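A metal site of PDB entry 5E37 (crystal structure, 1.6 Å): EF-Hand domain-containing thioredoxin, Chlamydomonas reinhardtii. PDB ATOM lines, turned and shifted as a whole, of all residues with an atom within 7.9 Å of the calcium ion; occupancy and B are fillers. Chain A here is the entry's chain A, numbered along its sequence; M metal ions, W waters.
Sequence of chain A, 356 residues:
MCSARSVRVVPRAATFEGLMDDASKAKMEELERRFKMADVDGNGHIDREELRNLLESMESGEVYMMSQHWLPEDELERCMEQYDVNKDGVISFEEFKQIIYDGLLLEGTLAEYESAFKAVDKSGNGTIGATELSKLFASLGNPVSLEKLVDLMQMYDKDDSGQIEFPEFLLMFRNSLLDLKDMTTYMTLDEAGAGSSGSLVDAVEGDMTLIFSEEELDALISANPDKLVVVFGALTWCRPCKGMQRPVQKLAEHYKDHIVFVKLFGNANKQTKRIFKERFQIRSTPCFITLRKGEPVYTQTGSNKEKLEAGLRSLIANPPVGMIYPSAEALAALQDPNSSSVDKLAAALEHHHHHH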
ATOM      1  N   PHE A  35      -4.377  14.485  -1.956  1.00  0.00           N
ATOM      2  CA  PHE A  35      -5.365  14.472  -0.951  1.00  0.00           C
ATOM      3  C   PHE A  35      -4.713  14.848   0.386  1.00  0.00           C
ATOM      4  O   PHE A  35      -5.308  15.645   1.138  1.00  0.00           O
ATOM      5  CB  PHE A  35      -6.015  13.080  -0.881  1.00  0.00           C
ATOM      6  CG  PHE A  35      -7.042  12.964   0.204  1.00  0.00           C
ATOM      7  CD1 PHE A  35      -8.288  13.540   0.094  1.00  0.00           C
ATOM      8  CD2 PHE A  35      -6.736  12.272   1.351  1.00  0.00           C
ATOM      9  CE1 PHE A  35      -9.285  13.429   1.050  1.00  0.00           C
ATOM     10  CE2 PHE A  35      -7.687  12.143   2.333  1.00  0.00           C
ATOM     11  CZ  PHE A  35      -8.966  12.734   2.216  1.00  0.00           C
ATOM     12  N   LYS A  36      -3.579  14.250   0.663  1.00  0.00           N
ATOM     13  CA  LYS A  36      -2.853  14.470   1.942  1.00  0.00           C
ATOM     14  C   LYS A  36      -2.418  15.945   2.057  1.00  0.00           C
ATOM     15  O   LYS A  36      -2.533  16.544   3.114  1.00  0.00           O
ATOM     16  CB  LYS A  36      -1.635  13.568   2.016  1.00  0.00           C
ATOM     17  CG  LYS A  36      -1.999  12.150   2.412  1.00  0.00           C
ATOM     18  CD  LYS A  36      -0.780  11.252   2.289  1.00  0.00           C
ATOM     19  CE  LYS A  36      -1.065   9.880   2.895  1.00  0.00           C
ATOM     20  NZ  LYS A  36      -0.457   8.804   2.070  1.00  0.00           N
ATOM     21  N   ALA A  38      -4.080  18.598   0.702  1.00  0.00           N
ATOM     22  CA  ALA A  38      -5.316  19.299   1.037  1.00  0.00           C
ATOM     23  C   ALA A  38      -5.760  19.060   2.456  1.00  0.00           C
ATOM     24  O   ALA A  38      -6.492  19.830   3.034  1.00  0.00           O
ATOM     25  CB  ALA A  38      -6.464  18.890   0.054  1.00  0.00           C
ATOM     26  N   ASP A  39      -5.420  17.892   2.969  1.00  0.00           N
ATOM     27  CA  ASP A  39      -5.764  17.554   4.357  1.00  0.00           C
ATOM     28  C   ASP A  39      -4.647  18.136   5.207  1.00  0.00           C
ATOM     29  O   ASP A  39      -3.730  17.441   5.645  1.00  0.00           O
ATOM     30  CB  ASP A  39      -5.868  16.026   4.518  1.00  0.00           C
ATOM     31  CG  ASP A  39      -6.266  15.595   5.931  1.00  0.00           C
ATOM     32  OD1 ASP A  39      -6.514  16.456   6.835  1.00  0.00           O
ATOM     33  OD2 ASP A  39      -6.373  14.369   6.106  1.00  0.00           O
ATOM     34  N   VAL A  40      -4.744  19.449   5.429  1.00  0.00           N
ATOM     35  CA  VAL A  40      -3.670  20.233   6.010  1.00  0.00           C
ATOM     36  C   VAL A  40      -3.297  19.768   7.398  1.00  0.00           C
ATOM     37  O   VAL A  40      -2.095  19.718   7.729  1.00  0.00           O
ATOM     38  CB  VAL A  40      -4.078  21.719   6.040  1.00  0.00           C
ATOM     39  CG1 VAL A  40      -3.163  22.605   6.906  1.00  0.00           C
ATOM     40  CG2 VAL A  40      -4.106  22.243   4.599  1.00  0.00           C
ATOM     41  N   ASP A  41      -4.301  19.456   8.206  1.00  0.00           N
ATOM     42  CA  ASP A  41      -3.990  19.105   9.601  1.00  0.00           C
ATOM     43  C   ASP A  41      -3.510  17.671   9.715  1.00  0.00           C
ATOM     44  O   ASP A  41      -3.118  17.250  10.795  1.00  0.00           O
ATOM     45  CB  ASP A  41      -5.147  19.393  10.584  1.00  0.00           C
ATOM     46  CG  ASP A  41      -6.399  18.629  10.271  1.00  0.00           C
ATOM     47  OD1 ASP A  41      -7.427  18.890  10.913  1.00  0.00           O
ATOM     48  OD2 ASP A  41      -6.393  17.783   9.354  1.00  0.00           O
ATOM     49  N   GLY A  42      -3.548  16.942   8.602  1.00  0.00           N
ATOM     50  CA  GLY A  42      -3.011  15.600   8.531  1.00  0.00           C
ATOM     51  C   GLY A  42      -3.963  14.655   9.219  1.00  0.00           C
ATOM     52  O   GLY A  42      -3.577  13.554   9.589  1.00  0.00           O
ATOM     53  N   ASN A  43      -5.213  15.050   9.394  1.00  0.00           N
ATOM     54  CA  ASN A  43      -6.102  14.234  10.208  1.00  0.00           C
ATOM     55  C   ASN A  43      -6.810  13.157   9.439  1.00  0.00           C
ATOM     56  O   ASN A  43      -7.786  12.611   9.930  1.00  0.00           O
ATOM     57  CB  ASN A  43      -7.114  15.091  10.980  1.00  0.00           C
ATOM     58  CG  ASN A  43      -8.404  15.368  10.199  1.00  0.00           C
ATOM     59  OD1 ASN A  43      -8.447  15.303   8.970  1.00  0.00           O
ATOM     60  ND2 ASN A  43      -9.462  15.685  10.919  1.00  0.00           N
ATOM     61  N   GLY A  44      -6.362  12.860   8.214  1.00  0.00           N
ATOM     62  CA  GLY A  44      -7.000  11.801   7.441  1.00  0.00           C
ATOM     63  C   GLY A  44      -8.201  12.182   6.595  1.00  0.00           C
ATOM     64  O   GLY A  44      -8.664  11.347   5.849  1.00  0.00           O
ATOM     65  N   HIS A  45      -8.725  13.413   6.662  1.00  0.00           N
ATOM     66  CA  HIS A  45      -9.852  13.828   5.785  1.00  0.00           C
ATOM     67  C   HIS A  45      -9.966  15.355   5.520  1.00  0.00           C
ATOM     68  O   HIS A  45      -9.272  16.093   6.172  1.00  0.00           O
ATOM     69  CB  HIS A  45     -11.160  13.252   6.305  1.00  0.00           C
ATOM     70  CG  HIS A  45     -11.652  13.881   7.570  1.00  0.00           C
ATOM     71  ND1 HIS A  45     -12.885  14.489   7.665  1.00  0.00           N
ATOM     72  CD2 HIS A  45     -11.106  13.932   8.805  1.00  0.00           C
ATOM     73  CE1 HIS A  45     -13.058  14.929   8.899  1.00  0.00           C
ATOM     74  NE2 HIS A  45     -11.991  14.609   9.609  1.00  0.00           N
ATOM     75  N   ILE A  46     -10.803  15.779   4.551  1.00  0.00           N
ATOM     76  CA  ILE A  46     -10.944  17.237   4.167  1.00  0.00           C
ATOM     77  C   ILE A  46     -12.244  17.862   4.696  1.00  0.00           C
ATOM     78  O   ILE A  46     -13.350  17.704   4.145  1.00  0.00           O
ATOM     79  CB  ILE A  46     -10.832  17.440   2.624  1.00  0.00           C
ATOM     80  CG1 ILE A  46      -9.473  16.951   2.131  1.00  0.00           C
ATOM     81  CG2 ILE A  46     -11.087  18.901   2.234  1.00  0.00           C
ATOM     82  CD1 ILE A  46      -9.435  16.910   0.613  1.00  0.00           C
ATOM     83  N   ASP A  47     -12.167  18.646   5.775  1.00  0.00           N
ATOM     84  CA  ASP A  47     -13.369  19.313   6.253  1.00  0.00           C
ATOM     85  C   ASP A  47     -13.708  20.563   5.436  1.00  0.00           C
ATOM     86  O   ASP A  47     -13.007  20.905   4.446  1.00  0.00           O
ATOM     87  CB  ASP A  47     -13.261  19.612   7.780  1.00  0.00           C
ATOM     88  CG  ASP A  47     -12.219  20.682   8.120  1.00  0.00           C
ATOM     89  OD1 ASP A  47     -12.129  21.693   7.389  1.00  0.00           O
ATOM     90  OD2 ASP A  47     -11.522  20.496   9.144  1.00  0.00           O
ATOM     91  N   ARG A  48     -14.819  21.191   5.828  1.00  0.00           N
ATOM     92  CA  ARG A  48     -15.433  22.272   5.104  1.00  0.00           C
ATOM     93  C   ARG A  48     -14.455  23.447   4.973  1.00  0.00           C
ATOM     94  O   ARG A  48     -14.270  24.022   3.885  1.00  0.00           O
ATOM     95  CB  ARG A  48     -16.703  22.680   5.829  1.00  0.00           C
ATOM     96  CG  ARG A  48     -17.574  23.603   5.068  1.00  0.00           C
ATOM     97  CD  ARG A  48     -19.019  23.488   5.509  1.00  0.00           C
ATOM     98  NE  ARG A  48     -19.840  24.286   4.591  1.00  0.00           N
ATOM     99  CZ  ARG A  48     -19.884  25.612   4.568  1.00  0.00           C
ATOM    100  NH1 ARG A  48     -19.209  26.363   5.462  1.00  0.00           N
ATOM    101  NH2 ARG A  48     -20.622  26.222   3.640  1.00  0.00           N
ATOM    102  N   GLU A  50     -11.060  23.241   5.220  1.00  0.00           N
ATOM    103  CA  GLU A  50      -9.938  22.838   4.391  1.00  0.00           C
ATOM    104  C   GLU A  50     -10.302  22.820   2.929  1.00  0.00           C
ATOM    105  O   GLU A  50      -9.504  23.061   2.026  1.00  0.00           O
ATOM    106  CB  GLU A  50      -9.437  21.413   4.738  1.00  0.00           C
ATOM    107  CG  GLU A  50      -8.948  21.295   6.170  1.00  0.00           C
ATOM    108  CD  GLU A  50      -8.729  19.862   6.614  1.00  0.00           C
ATOM    109  OE1 GLU A  50      -9.657  19.079   6.409  1.00  0.00           O
ATOM    110  OE2 GLU A  50      -7.657  19.589   7.213  1.00  0.00           O
ATOM    111  N   LEU A  51     -11.579  22.487   2.685  1.00  0.00           N
ATOM    112  CA  LEU A  51     -12.081  22.529   1.325  1.00  0.00           C
ATOM    113  C   LEU A  51     -12.214  24.010   0.828  1.00  0.00           C
ATOM    114  O   LEU A  51     -11.919  24.206  -0.340  1.00  0.00           O
ATOM    115  CB  LEU A  51     -13.468  21.798   1.286  1.00  0.00           C
ATOM    116  CG  LEU A  51     -14.121  21.866  -0.082  1.00  0.00           C
ATOM    117  CD1 LEU A  51     -13.443  20.851  -0.973  1.00  0.00           C
ATOM    118  CD2 LEU A  51     -15.596  21.538   0.095  1.00  0.00           C
ATOM    119  N   ILE A  91     -15.233  15.729   3.344  1.00  0.00           N
ATOM    120  CA  ILE A  91     -14.851  15.124   2.063  1.00  0.00           C
ATOM    121  C   ILE A  91     -13.827  14.028   2.271  1.00  0.00           C
ATOM    122  O   ILE A  91     -12.691  14.231   2.709  1.00  0.00           O
ATOM    123  CB  ILE A  91     -14.293  16.178   1.079  1.00  0.00           C
ATOM    124  CG1 ILE A  91     -15.370  17.191   0.661  1.00  0.00           C
ATOM    125  CG2 ILE A  91     -13.641  15.503  -0.133  1.00  0.00           C
ATOM    126  CD1 ILE A  91     -16.416  16.634  -0.253  1.00  0.00           C
HETATM  127 CA    CA M   1      -8.189  17.413   7.657  1.00  0.00          CA
HETATM  128  O   HOH W   1      -9.648  18.327   9.305  1.00  0.00           O
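The side-chain carboxylate of Asp 39 sits close to the backbone NH of Gly 42, at 3.5 Å.
The side-chain carboxylate of Asp 39 is in hydrogen-bond range of the backbone NH of Gly 44, 2.6 Å away.
N of Glu 50 is in hydrogen-bond range of OD1 of Asp 47.
OE2 of Glu 50 lies close to N of Val 40 (3.4 Å).
Within 4 Å of the calcium ion: Asp 39, Asp 41, Asn 43, His 45 and Glu 50.
The nearest printed residue that does not touch the calcium ion is Ile 46 (4.4 Å).
The calcium ion is bound by the side-chain carboxylate (OD1) of Asp 39 (2.1 Å), the backbone carbonyl oxygen (O) of His 45 (2.3 Å), the side-chain carboxylate (OE2) of Glu 50 (2.3 Å), water W1 (2.4 Å), the side-chain amide oxygen (OD1) of Asn 43 (2.5 Å), the side-chain carboxylate (OD2) of Asp 41 (2.5 Å) and the side-chain carboxylate (OE1) of Glu 50 (2.5 Å).
Water W1 lies within hydrogen-bond range of OD1 of Asp 41, OD2 of Asp 47 and ND2 of Asn 43.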
